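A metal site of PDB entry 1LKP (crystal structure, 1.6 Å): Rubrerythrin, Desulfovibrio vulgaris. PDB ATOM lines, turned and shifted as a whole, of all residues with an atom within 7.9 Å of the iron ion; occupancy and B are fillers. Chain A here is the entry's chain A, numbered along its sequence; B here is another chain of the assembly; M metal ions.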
ATOM      1  N   ARG A 157      21.152   9.159  -5.753  1.00  0.00           N
ATOM      2  CA  ARG A 157      19.923   9.437  -6.496  1.00  0.00           C
ATOM      3  C   ARG A 157      18.967   8.257  -6.426  1.00  0.00           C
ATOM      4  O   ARG A 157      19.370   7.101  -6.539  1.00  0.00           O
ATOM      5  CB  ARG A 157      20.239   9.731  -7.969  1.00  0.00           C
ATOM      6  CG  ARG A 157      19.021  10.233  -8.759  1.00  0.00           C
ATOM      7  CD  ARG A 157      19.315  10.370 -10.258  1.00  0.00           C
ATOM      8  NE  ARG A 157      19.441   9.065 -10.920  1.00  0.00           N
ATOM      9  CZ  ARG A 157      18.705   8.686 -11.959  1.00  0.00           C
ATOM     10  NH1 ARG A 157      17.784   9.497 -12.457  1.00  0.00           N
ATOM     11  NH2 ARG A 157      18.896   7.487 -12.503  1.00  0.00           N
ATOM     12  N   CYS A 158      17.683   8.552  -6.218  1.00  0.00           N
ATOM     13  CA  CYS A 158      16.667   7.511  -6.163  1.00  0.00           C
ATOM     14  C   CYS A 158      16.294   7.215  -7.620  1.00  0.00           C
ATOM     15  O   CYS A 158      15.798   8.096  -8.324  1.00  0.00           O
ATOM     16  CB  CYS A 158      15.431   8.000  -5.408  1.00  0.00           C
ATOM     17  SG  CYS A 158      14.038   6.856  -5.482  1.00  0.00           S
ATOM     18  N   ARG A 159      16.534   5.994  -8.067  1.00  0.00           N
ATOM     19  CA  ARG A 159      16.198   5.649  -9.452  1.00  0.00           C
ATOM     20  C   ARG A 159      14.695   5.683  -9.712  1.00  0.00           C
ATOM     21  O   ARG A 159      14.260   5.902 -10.840  1.00  0.00           O
ATOM     22  CB  ARG A 159      16.765   4.257  -9.805  1.00  0.00           C
ATOM     23  CG  ARG A 159      18.285   4.231  -9.955  1.00  0.00           C
ATOM     24  CD  ARG A 159      18.790   2.845 -10.380  1.00  0.00           C
ATOM     25  NE  ARG A 159      18.297   2.461 -11.705  1.00  0.00           N
ATOM     26  CZ  ARG A 159      18.703   3.001 -12.854  1.00  0.00           C
ATOM     27  NH1 ARG A 159      19.633   3.956 -12.869  1.00  0.00           N
ATOM     28  NH2 ARG A 159      18.174   2.584 -14.000  1.00  0.00           N
ATOM     29  N   ASN A 160      13.895   5.486  -8.670  1.00  0.00           N
ATOM     30  CA  ASN A 160      12.437   5.481  -8.832  1.00  0.00           C
ATOM     31  C   ASN A 160      11.818   6.861  -9.092  1.00  0.00           C
ATOM     32  O   ASN A 160      10.927   6.982  -9.953  1.00  0.00           O
ATOM     33  CB  ASN A 160      11.756   4.867  -7.610  1.00  0.00           C
ATOM     34  CG  ASN A 160      10.268   4.642  -7.813  1.00  0.00           C
ATOM     35  OD1 ASN A 160       9.429   5.252  -7.137  1.00  0.00           O
ATOM     36  ND2 ASN A 160       9.933   3.764  -8.755  1.00  0.00           N
ATOM     37  N   CYS A 161      12.284   7.881  -8.390  1.00  0.00           N
ATOM     38  CA  CYS A 161      11.711   9.222  -8.551  1.00  0.00           C
ATOM     39  C   CYS A 161      12.687  10.369  -8.785  1.00  0.00           C
ATOM     40  O   CYS A 161      12.269  11.500  -9.013  1.00  0.00           O
ATOM     41  CB  CYS A 161      10.852   9.568  -7.332  1.00  0.00           C
ATOM     42  SG  CYS A 161      11.821  10.016  -5.860  1.00  0.00           S
ATOM     43  N   GLY A 162      13.984  10.084  -8.725  1.00  0.00           N
ATOM     44  CA  GLY A 162      14.953  11.140  -8.965  1.00  0.00           C
ATOM     45  C   GLY A 162      15.389  11.963  -7.760  1.00  0.00           C
ATOM     46  O   GLY A 162      16.178  12.890  -7.905  1.00  0.00           O
ATOM     47  N   TYR A 163      14.864  11.659  -6.583  1.00  0.00           N
ATOM     48  CA  TYR A 163      15.252  12.401  -5.385  1.00  0.00           C
ATOM     49  C   TYR A 163      16.766  12.284  -5.191  1.00  0.00           C
ATOM     50  O   TYR A 163      17.353  11.236  -5.441  1.00  0.00           O
ATOM     51  CB  TYR A 163      14.541  11.851  -4.151  1.00  0.00           C
ATOM     52  CG  TYR A 163      14.950  12.544  -2.873  1.00  0.00           C
ATOM     53  CD1 TYR A 163      14.505  13.826  -2.581  1.00  0.00           C
ATOM     54  CD2 TYR A 163      15.831  11.928  -1.981  1.00  0.00           C
ATOM     55  CE1 TYR A 163      14.927  14.491  -1.422  1.00  0.00           C
ATOM     56  CE2 TYR A 163      16.273  12.586  -0.833  1.00  0.00           C
ATOM     57  CZ  TYR A 163      15.813  13.862  -0.557  1.00  0.00           C
ATOM     58  OH  TYR A 163      16.224  14.514   0.584  1.00  0.00           O
ATOM     59  N   VAL A 164      17.387  13.365  -4.736  1.00  0.00           N
ATOM     60  CA  VAL A 164      18.819  13.363  -4.494  1.00  0.00           C
ATOM     61  C   VAL A 164      19.062  13.522  -3.004  1.00  0.00           C
ATOM     62  O   VAL A 164      18.577  14.478  -2.374  1.00  0.00           O
ATOM     63  CB  VAL A 164      19.512  14.522  -5.245  1.00  0.00           C
ATOM     64  CG1 VAL A 164      21.007  14.526  -4.925  1.00  0.00           C
ATOM     65  CG2 VAL A 164      19.297  14.360  -6.743  1.00  0.00           C
ATOM     66  N   LEU A 173      14.540   4.836   3.397  1.00  0.00           N
ATOM     67  CA  LEU A 173      13.344   5.094   2.595  1.00  0.00           C
ATOM     68  C   LEU A 173      13.498   6.441   1.904  1.00  0.00           C
ATOM     69  O   LEU A 173      13.989   7.397   2.506  1.00  0.00           O
ATOM     70  CB  LEU A 173      12.097   5.132   3.477  1.00  0.00           C
ATOM     71  CG  LEU A 173      11.596   3.807   4.064  1.00  0.00           C
ATOM     72  CD1 LEU A 173      10.368   4.075   4.935  1.00  0.00           C
ATOM     73  CD2 LEU A 173      11.238   2.836   2.938  1.00  0.00           C
ATOM     74  N   CYS A 174      13.097   6.514   0.643  1.00  0.00           N
ATOM     75  CA  CYS A 174      13.193   7.763  -0.098  1.00  0.00           C
ATOM     76  C   CYS A 174      12.160   8.735   0.485  1.00  0.00           C
ATOM     77  O   CYS A 174      10.981   8.420   0.592  1.00  0.00           O
ATOM     78  CB  CYS A 174      12.894   7.527  -1.584  1.00  0.00           C
ATOM     79  SG  CYS A 174      12.912   9.049  -2.560  1.00  0.00           S
ATOM     80  N   PRO A 175      12.601   9.936   0.887  1.00  0.00           N
ATOM     81  CA  PRO A 175      11.645  10.892   1.452  1.00  0.00           C
ATOM     82  C   PRO A 175      10.608  11.418   0.468  1.00  0.00           C
ATOM     83  O   PRO A 175       9.584  11.976   0.878  1.00  0.00           O
ATOM     84  CB  PRO A 175      12.544  11.992   2.008  1.00  0.00           C
ATOM     85  CG  PRO A 175      13.709  11.968   1.066  1.00  0.00           C
ATOM     86  CD  PRO A 175      13.968  10.479   0.902  1.00  0.00           C
ATOM     87  N   ALA A 176      10.864  11.249  -0.825  1.00  0.00           N
ATOM     88  CA  ALA A 176       9.928  11.705  -1.846  1.00  0.00           C
ATOM     89  C   ALA A 176       8.908  10.636  -2.253  1.00  0.00           C
ATOM     90  O   ALA A 176       7.709  10.848  -2.112  1.00  0.00           O
ATOM     91  CB  ALA A 176      10.699  12.172  -3.085  1.00  0.00           C
ATOM     92  N   CYS A 177       9.378   9.492  -2.723  1.00  0.00           N
ATOM     93  CA  CYS A 177       8.478   8.432  -3.174  1.00  0.00           C
ATOM     94  C   CYS A 177       8.249   7.270  -2.208  1.00  0.00           C
ATOM     95  O   CYS A 177       7.486   6.346  -2.517  1.00  0.00           O
ATOM     96  CB  CYS A 177       8.957   7.881  -4.521  1.00  0.00           C
ATOM     97  SG  CYS A 177      10.436   6.847  -4.401  1.00  0.00           S
ATOM     98  N   ALA A 178       8.912   7.302  -1.063  1.00  0.00           N
ATOM     99  CA  ALA A 178       8.768   6.257  -0.046  1.00  0.00           C
ATOM    100  C   ALA A 178       9.249   4.867  -0.433  1.00  0.00           C
ATOM    101  O   ALA A 178       8.937   3.891   0.250  1.00  0.00           O
ATOM    102  CB  ALA A 178       7.309   6.195   0.425  1.00  0.00           C
ATOM    103  N   HIS A 179       9.983   4.751  -1.539  1.00  0.00           N
ATOM    104  CA  HIS A 179      10.492   3.445  -1.931  1.00  0.00           C
ATOM    105  C   HIS A 179      11.755   3.139  -1.107  1.00  0.00           C
ATOM    106  O   HIS A 179      12.407   4.052  -0.610  1.00  0.00           O
ATOM    107  CB  HIS A 179      10.769   3.393  -3.424  1.00  0.00           C
ATOM    108  CG  HIS A 179       9.531   3.201  -4.245  1.00  0.00           C
ATOM    109  ND1 HIS A 179       8.417   4.002  -4.118  1.00  0.00           N
ATOM    110  CD2 HIS A 179       9.221   2.276  -5.181  1.00  0.00           C
ATOM    111  CE1 HIS A 179       7.480   3.578  -4.941  1.00  0.00           C
ATOM    112  NE2 HIS A 179       7.929   2.529  -5.593  1.00  0.00           N
ATOM    113  N   PRO A 180      12.094   1.850  -0.946  1.00  0.00           N
ATOM    114  CA  PRO A 180      13.266   1.460  -0.170  1.00  0.00           C
ATOM    115  C   PRO A 180      14.639   1.816  -0.726  1.00  0.00           C
ATOM    116  O   PRO A 180      14.799   2.111  -1.914  1.00  0.00           O
ATOM    117  CB  PRO A 180      13.080  -0.042   0.003  1.00  0.00           C
ATOM    118  CG  PRO A 180      12.386  -0.435  -1.255  1.00  0.00           C
ATOM    119  CD  PRO A 180      11.369   0.663  -1.448  1.00  0.00           C
ATOM    120  N   HIS A 183      16.484   1.308  -4.228  1.00  0.00           N
ATOM    121  CA  HIS A 183      16.390   2.116  -5.443  1.00  0.00           C
ATOM    122  C   HIS A 183      17.491   3.157  -5.628  1.00  0.00           C
ATOM    123  O   HIS A 183      17.587   3.781  -6.687  1.00  0.00           O
ATOM    124  CB  HIS A 183      15.027   2.794  -5.500  1.00  0.00           C
ATOM    125  CG  HIS A 183      13.885   1.832  -5.681  1.00  0.00           C
ATOM    126  ND1 HIS A 183      13.364   1.527  -6.921  1.00  0.00           N
ATOM    127  CD2 HIS A 183      13.223   1.065  -4.795  1.00  0.00           C
ATOM    128  CE1 HIS A 183      12.426   0.612  -6.781  1.00  0.00           C
ATOM    129  NE2 HIS A 183      12.319   0.311  -5.500  1.00  0.00           N
ATOM    130  N   PHE A 184      18.329   3.349  -4.610  1.00  0.00           N
ATOM    131  CA  PHE A 184      19.376   4.362  -4.705  1.00  0.00           C
ATOM    132  C   PHE A 184      20.685   3.946  -5.376  1.00  0.00           C
ATOM    133  O   PHE A 184      21.095   2.783  -5.338  1.00  0.00           O
ATOM    134  CB  PHE A 184      19.681   4.938  -3.326  1.00  0.00           C
ATOM    135  CG  PHE A 184      18.621   5.878  -2.816  1.00  0.00           C
ATOM    136  CD1 PHE A 184      17.476   5.390  -2.185  1.00  0.00           C
ATOM    137  CD2 PHE A 184      18.756   7.258  -2.993  1.00  0.00           C
ATOM    138  CE1 PHE A 184      16.474   6.257  -1.752  1.00  0.00           C
ATOM    139  CE2 PHE A 184      17.751   8.137  -2.566  1.00  0.00           C
ATOM    140  CZ  PHE A 184      16.616   7.633  -1.940  1.00  0.00           C
ATOM    141  N   GLN B  52       9.710   8.930 -13.678  1.00  0.00           N
ATOM    142  CA  GLN B  52       9.864   9.451 -12.332  1.00  0.00           C
ATOM    143  C   GLN B  52       8.711  10.396 -11.996  1.00  0.00           C
ATOM    144  O   GLN B  52       8.277  10.440 -10.846  1.00  0.00           O
ATOM    145  CB  GLN B  52      11.233  10.114 -12.180  1.00  0.00           C
ATOM    146  CG  GLN B  52      12.359   9.101 -12.405  1.00  0.00           C
ATOM    147  CD  GLN B  52      13.752   9.633 -12.185  1.00  0.00           C
ATOM    148  OE1 GLN B  52      14.021  10.811 -12.384  1.00  0.00           O
ATOM    149  NE2 GLN B  52      14.674   8.744 -11.796  1.00  0.00           N
ATOM    150  N   GLU B  55       5.971   8.495 -10.728  1.00  0.00           N
ATOM    151  CA  GLU B  55       6.151   8.136  -9.322  1.00  0.00           C
ATOM    152  C   GLU B  55       5.828   9.300  -8.374  1.00  0.00           C
ATOM    153  O   GLU B  55       5.341   9.086  -7.274  1.00  0.00           O
ATOM    154  CB  GLU B  55       7.555   7.592  -9.093  1.00  0.00           C
ATOM    155  CG  GLU B  55       7.808   6.283  -9.861  1.00  0.00           C
ATOM    156  CD  GLU B  55       6.836   5.178  -9.477  1.00  0.00           C
ATOM    157  OE1 GLU B  55       6.608   4.966  -8.263  1.00  0.00           O
ATOM    158  OE2 GLU B  55       6.298   4.491 -10.388  1.00  0.00           O
ATOM    159  N   HIS B  56       6.125  10.530  -8.789  1.00  0.00           N
ATOM    160  CA  HIS B  56       5.779  11.677  -7.949  1.00  0.00           C
ATOM    161  C   HIS B  56       4.253  11.696  -7.869  1.00  0.00           C
ATOM    162  O   HIS B  56       3.674  11.881  -6.800  1.00  0.00           O
ATOM    163  CB  HIS B  56       6.230  12.997  -8.589  1.00  0.00           C
ATOM    164  CG  HIS B  56       7.704  13.145  -8.715  1.00  0.00           C
ATOM    165  ND1 HIS B  56       8.287  14.150  -9.458  1.00  0.00           N
ATOM    166  CD2 HIS B  56       8.730  12.405  -8.216  1.00  0.00           C
ATOM    167  CE1 HIS B  56       9.609  14.025  -9.414  1.00  0.00           C
ATOM    168  NE2 HIS B  56       9.896  12.974  -8.668  1.00  0.00           N
ATOM    169  N   ARG B  59       2.744   9.005  -5.515  1.00  0.00           N
ATOM    170  CA  ARG B  59       2.872   9.335  -4.100  1.00  0.00           C
ATOM    171  C   ARG B  59       1.781  10.334  -3.722  1.00  0.00           C
ATOM    172  O   ARG B  59       1.125  10.190  -2.693  1.00  0.00           O
ATOM    173  CB  ARG B  59       4.252   9.946  -3.804  1.00  0.00           C
ATOM    174  CG  ARG B  59       4.497  10.232  -2.315  1.00  0.00           C
ATOM    175  CD  ARG B  59       4.636   8.937  -1.517  1.00  0.00           C
ATOM    176  NE  ARG B  59       4.470   9.108  -0.079  1.00  0.00           N
ATOM    177  CZ  ARG B  59       5.423   9.485   0.771  1.00  0.00           C
ATOM    178  NH1 ARG B  59       6.645   9.748   0.340  1.00  0.00           N
ATOM    179  NH2 ARG B  59       5.149   9.580   2.063  1.00  0.00           N
ATOM    180  N   SER B 123      10.544  17.331  -0.826  1.00  0.00           N
ATOM    181  CA  SER B 123      11.404  16.285  -1.354  1.00  0.00           C
ATOM    182  C   SER B 123      11.254  16.146  -2.866  1.00  0.00           C
ATOM    183  O   SER B 123      12.228  15.968  -3.583  1.00  0.00           O
ATOM    184  CB  SER B 123      11.095  14.957  -0.665  1.00  0.00           C
ATOM    185  OG  SER B 123      11.420  15.043   0.718  1.00  0.00           O
ATOM    186  N   ALA B 127      13.963  16.559  -6.450  1.00  0.00           N
ATOM    187  CA  ALA B 127      14.037  15.736  -7.661  1.00  0.00           C
ATOM    188  C   ALA B 127      13.893  16.606  -8.901  1.00  0.00           C
ATOM    189  O   ALA B 127      14.640  16.443  -9.873  1.00  0.00           O
ATOM    190  CB  ALA B 127      12.932  14.685  -7.645  1.00  0.00           C
HETATM  191 FE    FE M   1      12.327   8.201  -4.617  1.00  0.00          FE
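The side-chain sulfur (SG) of Cys 161 sits close to the backbone NH (N) of Tyr 163 (3.5 Å). O of Cys 161 is in hydrogen-bond range of NE2 of His 56 of chain B, at 2.8 Å. The backbone NH (N) of Ala 176 sits close to the side-chain sulfur (SG) of Cys 174 (3.5 Å). The backbone NH (N) of Cys 174 is in hydrogen-bond range of the backbone carbonyl oxygen (O) of His 179 (2.8 Å). The side-chain sulfur (SG) of Cys 177 sits close to the side-chain amide oxygen (OD1) of Asn 160 (3.3 Å). The backbone carbonyl oxygen of Cys 177 lies within hydrogen-bond range of a ring nitrogen (ND1) of His 179 (3.0 Å). The backbone carbonyl oxygen (O) of Tyr 163 is in hydrogen-bond range of the backbone NH (N) of Cys 158. The side-chain sulfur (SG) of Cys 158 lies close to the backbone NH (N) of Asn 160.
SG of Cys 161 binds the iron ion (2.3 Å). The iron ion is bound by the side-chain sulfur (SG) of Cys 174. SG of Cys 177 binds the iron ion, at 2.3 Å. SG of Cys 158 binds the iron ion.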
